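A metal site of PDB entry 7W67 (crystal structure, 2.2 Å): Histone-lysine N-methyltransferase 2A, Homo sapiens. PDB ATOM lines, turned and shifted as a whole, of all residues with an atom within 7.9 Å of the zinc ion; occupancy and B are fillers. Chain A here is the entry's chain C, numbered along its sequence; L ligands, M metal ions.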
ATOM      1  N   ILE A  26     -22.501  28.896  -1.791  1.00  0.00           N
ATOM      2  CA  ILE A  26     -23.148  27.888  -0.970  1.00  0.00           C
ATOM      3  C   ILE A  26     -22.289  26.641  -0.887  1.00  0.00           C
ATOM      4  O   ILE A  26     -21.948  26.167   0.205  1.00  0.00           O
ATOM      5  CB  ILE A  26     -24.547  27.572  -1.524  1.00  0.00           C
ATOM      6  CG1 ILE A  26     -25.435  28.821  -1.449  1.00  0.00           C
ATOM      7  CG2 ILE A  26     -25.153  26.390  -0.778  1.00  0.00           C
ATOM      8  CD1 ILE A  26     -26.813  28.639  -2.036  1.00  0.00           C
ATOM      9  N   HIS A  96     -29.205  23.320  -2.569  1.00  0.00           N
ATOM     10  CA  HIS A  96     -30.303  23.457  -1.628  1.00  0.00           C
ATOM     11  C   HIS A  96     -30.229  24.793  -0.896  1.00  0.00           C
ATOM     12  O   HIS A  96     -29.160  25.268  -0.565  1.00  0.00           O
ATOM     13  CB  HIS A  96     -30.285  22.317  -0.600  1.00  0.00           C
ATOM     14  CG  HIS A  96     -31.153  22.552   0.588  1.00  0.00           C
ATOM     15  ND1 HIS A  96     -32.426  22.035   0.699  1.00  0.00           N
ATOM     16  CD2 HIS A  96     -30.931  23.245   1.734  1.00  0.00           C
ATOM     17  CE1 HIS A  96     -32.954  22.407   1.855  1.00  0.00           C
ATOM     18  NE2 HIS A  96     -32.073  23.143   2.497  1.00  0.00           N
ATOM     19  N   SER A  97     -31.397  25.366  -0.620  1.00  0.00           N
ATOM     20  CA  SER A  97     -31.503  26.498   0.289  1.00  0.00           C
ATOM     21  C   SER A  97     -32.732  26.341   1.160  1.00  0.00           C
ATOM     22  O   SER A  97     -33.726  25.741   0.750  1.00  0.00           O
ATOM     23  CB  SER A  97     -31.553  27.854  -0.433  1.00  0.00           C
ATOM     24  OG  SER A  97     -31.958  28.888   0.451  1.00  0.00           O
ATOM     25  N   CYS A  98     -32.662  26.902   2.373  1.00  0.00           N
ATOM     26  CA  CYS A  98     -33.793  26.901   3.299  1.00  0.00           C
ATOM     27  C   CYS A  98     -34.776  28.028   2.996  1.00  0.00           C
ATOM     28  O   CYS A  98     -35.941  27.938   3.382  1.00  0.00           O
ATOM     29  CB  CYS A  98     -33.293  27.016   4.735  1.00  0.00           C
ATOM     30  SG  CYS A  98     -32.194  25.689   5.257  1.00  0.00           S
ATOM     31  N   GLU A  99     -34.314  29.090   2.330  1.00  0.00           N
ATOM     32  CA  GLU A  99     -35.190  30.133   1.793  1.00  0.00           C
ATOM     33  C   GLU A  99     -35.018  30.163   0.273  1.00  0.00           C
ATOM     34  O   GLU A  99     -34.565  31.162  -0.300  1.00  0.00           O
ATOM     35  CB  GLU A  99     -34.890  31.492   2.409  1.00  0.00           C
ATOM     36  CG  GLU A  99     -35.304  31.657   3.878  1.00  0.00           C
ATOM     37  CD  GLU A  99     -35.578  33.121   4.253  1.00  0.00           C
ATOM     38  OE1 GLU A  99     -36.664  33.399   4.808  1.00  0.00           O
ATOM     39  OE2 GLU A  99     -34.716  33.990   3.982  1.00  0.00           O
ATOM     40  N   PRO A 145     -24.519  19.413   7.084  1.00  0.00           N
ATOM     41  CA  PRO A 145     -24.795  20.790   7.513  1.00  0.00           C
ATOM     42  C   PRO A 145     -25.057  21.689   6.319  1.00  0.00           C
ATOM     43  O   PRO A 145     -24.400  21.604   5.281  1.00  0.00           O
ATOM     44  CB  PRO A 145     -23.514  21.184   8.253  1.00  0.00           C
ATOM     45  CG  PRO A 145     -22.442  20.401   7.566  1.00  0.00           C
ATOM     46  CD  PRO A 145     -23.076  19.102   7.099  1.00  0.00           C
ATOM     47  N   CYS A 146     -26.040  22.576   6.487  1.00  0.00           N
ATOM     48  CA  CYS A 146     -26.440  23.486   5.423  1.00  0.00           C
ATOM     49  C   CYS A 146     -25.603  24.754   5.443  1.00  0.00           C
ATOM     50  O   CYS A 146     -25.470  25.399   6.489  1.00  0.00           O
ATOM     51  CB  CYS A 146     -27.927  23.833   5.555  1.00  0.00           C
ATOM     52  SG  CYS A 146     -28.501  24.769   4.144  1.00  0.00           S
ATOM     53  N   ASN A 147     -25.067  25.123   4.273  1.00  0.00           N
ATOM     54  CA  ASN A 147     -24.341  26.377   4.084  1.00  0.00           C
ATOM     55  C   ASN A 147     -25.101  27.318   3.136  1.00  0.00           C
ATOM     56  O   ASN A 147     -24.483  28.048   2.357  1.00  0.00           O
ATOM     57  CB  ASN A 147     -22.925  26.115   3.558  1.00  0.00           C
ATOM     58  CG  ASN A 147     -21.988  27.311   3.744  1.00  0.00           C
ATOM     59  OD1 ASN A 147     -21.934  27.912   4.825  1.00  0.00           O
ATOM     60  ND2 ASN A 147     -21.232  27.647   2.701  1.00  0.00           N
ATOM     61  N   CYS A 148     -26.437  27.319   3.200  1.00  0.00           N
ATOM     62  CA  CYS A 148     -27.208  28.094   2.223  1.00  0.00           C
ATOM     63  C   CYS A 148     -27.141  29.592   2.503  1.00  0.00           C
ATOM     64  O   CYS A 148     -27.378  30.398   1.602  1.00  0.00           O
ATOM     65  CB  CYS A 148     -28.661  27.636   2.207  1.00  0.00           C
ATOM     66  SG  CYS A 148     -29.635  28.115   3.667  1.00  0.00           S
ATOM     67  N   GLY A 149     -26.837  29.983   3.747  1.00  0.00           N
ATOM     68  CA  GLY A 149     -26.711  31.376   4.097  1.00  0.00           C
ATOM     69  C   GLY A 149     -28.012  32.090   4.406  1.00  0.00           C
ATOM     70  O   GLY A 149     -27.970  33.279   4.740  1.00  0.00           O
ATOM     71  N   ALA A 150     -29.154  31.417   4.296  1.00  0.00           N
ATOM     72  CA  ALA A 150     -30.405  32.065   4.628  1.00  0.00           C
ATOM     73  C   ALA A 150     -30.451  32.425   6.114  1.00  0.00           C
ATOM     74  O   ALA A 150     -29.835  31.760   6.961  1.00  0.00           O
ATOM     75  CB  ALA A 150     -31.590  31.174   4.263  1.00  0.00           C
ATOM     76  N   LYS A 151     -31.169  33.494   6.434  1.00  0.00           N
ATOM     77  CA  LYS A 151     -31.397  33.840   7.833  1.00  0.00           C
ATOM     78  C   LYS A 151     -32.297  32.845   8.546  1.00  0.00           C
ATOM     79  O   LYS A 151     -32.289  32.776   9.768  1.00  0.00           O
ATOM     80  CB  LYS A 151     -31.999  35.249   7.938  1.00  0.00           C
ATOM     81  CG  LYS A 151     -33.439  35.329   7.456  1.00  0.00           C
ATOM     82  CD  LYS A 151     -33.896  36.776   7.339  1.00  0.00           C
ATOM     83  CE  LYS A 151     -35.409  36.872   7.241  1.00  0.00           C
ATOM     84  NZ  LYS A 151     -36.056  36.940   8.593  1.00  0.00           N
ATOM     85  N   LYS A 152     -33.080  32.087   7.789  1.00  0.00           N
ATOM     86  CA  LYS A 152     -33.967  31.072   8.340  1.00  0.00           C
ATOM     87  C   LYS A 152     -33.415  29.668   8.093  1.00  0.00           C
ATOM     88  O   LYS A 152     -34.166  28.720   7.848  1.00  0.00           O
ATOM     89  CB  LYS A 152     -35.366  31.227   7.752  1.00  0.00           C
ATOM     90  CG  LYS A 152     -36.144  32.439   8.243  1.00  0.00           C
ATOM     91  CD  LYS A 152     -36.677  32.240   9.646  1.00  0.00           C
ATOM     92  CE  LYS A 152     -37.878  33.160   9.845  1.00  0.00           C
ATOM     93  NZ  LYS A 152     -37.640  34.282  10.786  1.00  0.00           N
ATOM     94  N   CYS A 153     -32.098  29.533   8.178  1.00  0.00           N
ATOM     95  CA  CYS A 153     -31.453  28.272   7.826  1.00  0.00           C
ATOM     96  C   CYS A 153     -31.653  27.218   8.909  1.00  0.00           C
ATOM     97  O   CYS A 153     -31.411  27.472  10.094  1.00  0.00           O
ATOM     98  CB  CYS A 153     -29.958  28.504   7.599  1.00  0.00           C
ATOM     99  SG  CYS A 153     -29.031  26.985   7.322  1.00  0.00           S
ATOM    100  N   ARG A 154     -32.060  26.037   8.497  1.00  0.00           N
ATOM    101  CA  ARG A 154     -32.268  24.933   9.413  1.00  0.00           C
ATOM    102  C   ARG A 154     -31.026  24.159   9.755  1.00  0.00           C
ATOM    103  O   ARG A 154     -31.095  23.160  10.432  1.00  0.00           O
ATOM    104  CB  ARG A 154     -33.277  23.961   8.835  1.00  0.00           C
ATOM    105  CG  ARG A 154     -34.544  24.617   8.384  1.00  0.00           C
ATOM    106  CD  ARG A 154     -35.438  23.655   7.639  1.00  0.00           C
ATOM    107  NE  ARG A 154     -36.476  24.390   6.959  1.00  0.00           N
ATOM    108  CZ  ARG A 154     -36.478  24.640   5.666  1.00  0.00           C
ATOM    109  NH1 ARG A 154     -37.449  25.328   5.115  1.00  0.00           N
ATOM    110  NH2 ARG A 154     -35.497  24.178   4.913  1.00  0.00           N
ATOM    111  N   LYS A 155     -29.901  24.598   9.207  1.00  0.00           N
ATOM    112  CA  LYS A 155     -28.543  24.144   9.513  1.00  0.00           C
ATOM    113  C   LYS A 155     -28.088  22.767   9.027  1.00  0.00           C
ATOM    114  O   LYS A 155     -26.925  22.499   8.962  1.00  0.00           O
ATOM    115  CB  LYS A 155     -28.175  24.370  10.981  1.00  0.00           C
ATOM    116  CG  LYS A 155     -28.574  25.746  11.485  1.00  0.00           C
ATOM    117  CD  LYS A 155     -28.293  25.873  12.973  1.00  0.00           C
ATOM    118  CE  LYS A 155     -27.317  26.985  13.305  1.00  0.00           C
ATOM    119  NZ  LYS A 155     -27.101  27.086  14.776  1.00  0.00           N
ATOM    120  N   PHE A 156     -29.013  21.883   8.675  1.00  0.00           N
ATOM    121  CA  PHE A 156     -28.675  20.699   7.876  1.00  0.00           C
ATOM    122  C   PHE A 156     -29.637  20.549   6.709  1.00  0.00           C
ATOM    123  O   PHE A 156     -30.747  21.015   6.752  1.00  0.00           O
ATOM    124  CB  PHE A 156     -28.710  19.405   8.712  1.00  0.00           C
ATOM    125  CG  PHE A 156     -28.270  19.589  10.128  1.00  0.00           C
ATOM    126  CD1 PHE A 156     -26.954  19.485  10.460  1.00  0.00           C
ATOM    127  CD2 PHE A 156     -29.182  19.959  11.079  1.00  0.00           C
ATOM    128  CE1 PHE A 156     -26.543  19.698  11.746  1.00  0.00           C
ATOM    129  CE2 PHE A 156     -28.781  20.161  12.381  1.00  0.00           C
ATOM    130  CZ  PHE A 156     -27.469  20.044  12.713  1.00  0.00           C
ATOM    131  N   LEU A 157     -29.210  19.846   5.679  1.00  0.00           N
ATOM    132  CA  LEU A 157     -30.142  19.329   4.697  1.00  0.00           C
ATOM    133  C   LEU A 157     -31.031  18.226   5.258  1.00  0.00           C
ATOM    134  O   LEU A 157     -32.109  18.018   4.769  1.00  0.00           O
ATOM    135  CB  LEU A 157     -29.409  18.846   3.459  1.00  0.00           C
ATOM    136  CG  LEU A 157     -28.151  19.600   3.059  1.00  0.00           C
ATOM    137  CD1 LEU A 157     -27.513  18.998   1.833  1.00  0.00           C
ATOM    138  CD2 LEU A 157     -28.429  21.054   2.777  1.00  0.00           C
HETATM  139  N1  LIG L   1     -22.933  22.011  -5.262  1.00  0.00           N
HETATM  140  C1  LIG L   1     -22.680  20.800  -6.024  1.00  0.00           C
HETATM  141  C2  LIG L   1     -23.853  20.551  -6.951  1.00  0.00           C
HETATM  142  C3  LIG L   1     -25.126  20.163  -6.219  1.00  0.00           C
HETATM  143  S1  LIG L   1     -25.273  18.366  -6.123  1.00  0.00           S
HETATM  144  C4  LIG L   1     -21.383  20.902  -6.803  1.00  0.00           C
HETATM  145  O1  LIG L   1     -20.531  21.726  -6.462  1.00  0.00           O
HETATM  146  O2  LIG L   1     -21.151  20.182  -7.781  1.00  0.00           O
HETATM  147  C5  LIG L   1     -25.785  18.435  -4.386  1.00  0.00           C
HETATM  148  C6  LIG L   1     -24.587  18.391  -3.443  1.00  0.00           C
HETATM  149  O3  LIG L   1     -24.164  19.713  -3.200  1.00  0.00           O
HETATM  150  C7  LIG L   1     -24.955  17.754  -2.117  1.00  0.00           C
HETATM  151  O4  LIG L   1     -24.406  16.457  -2.026  1.00  0.00           O
HETATM  152  C8  LIG L   1     -24.366  18.688  -1.068  1.00  0.00           C
HETATM  153  O5  LIG L   1     -23.196  18.186  -0.482  1.00  0.00           O
HETATM  154  C9  LIG L   1     -23.993  19.945  -1.814  1.00  0.00           C
HETATM  155  N2  LIG L   1     -24.935  20.976  -1.350  1.00  0.00           N
HETATM  156  C10 LIG L   1     -26.129  21.285  -1.935  1.00  0.00           C
HETATM  157  N3  LIG L   1     -26.724  22.255  -1.204  1.00  0.00           N
HETATM  158  C11 LIG L   1     -25.921  22.561  -0.149  1.00  0.00           C
HETATM  159  C12 LIG L   1     -26.053  23.473   0.891  1.00  0.00           C
HETATM  160  N4  LIG L   1     -27.112  24.256   0.990  1.00  0.00           N
HETATM  161  N5  LIG L   1     -25.051  23.551   1.843  1.00  0.00           N
HETATM  162  C13 LIG L   1     -23.935  22.745   1.739  1.00  0.00           C
HETATM  163  N6  LIG L   1     -23.820  21.845   0.710  1.00  0.00           N
HETATM  164  C14 LIG L   1     -24.791  21.750  -0.228  1.00  0.00           C
HETATM  165 ZN    ZN M   1     -29.856  26.230   5.029  1.00  0.00          ZN
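O of Lys 155 is in hydrogen-bond range of N of Cys 146 (2.6 Å).
SG of Cys 148 sits close to N of Ala 150 (3.4 Å).
The guanidinium group (NH1) of Arg 154 sits at hydrogen-bond distance from the backbone carbonyl oxygen (O) of Cys 98 (3.5 Å).
A ring nitrogen (NE2) of His 96 lies close to the side-chain sulfur (SG) of Cys 98, 3.8 Å away.
The side-chain sulfur of Cys 153 lies close to the backbone NH of Lys 155, 3.2 Å away.
The side-chain sulfur (SG) of Cys 146 sits close to a nitrogen (N4) of the ligand, 3.5 Å away.
N of His 96 is in hydrogen-bond range of N3 of the ligand (3.0 Å).
The backbone carbonyl oxygen (O) of His 96 lies within hydrogen-bond range of a nitrogen (N4) of the ligand, at 2.8 Å.
The backbone NH of Asn 147 lies within hydrogen-bond range of a nitrogen (N5) of the ligand (2.9 Å).
Within 4 Å of the zinc ion: Cys 98, Cys 146, Cys 148 and Cys 153.
The nearest printed residue that does not touch the zinc ion is Arg 154 (4.1 Å).
The zinc ion is bound by the side-chain sulfur of Cys 146 (2.2 Å), the side-chain sulfur of Cys 148 (2.3 Å), the side-chain sulfur of Cys 98 (2.4 Å) and the side-chain sulfur of Cys 153 (2.6 Å).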
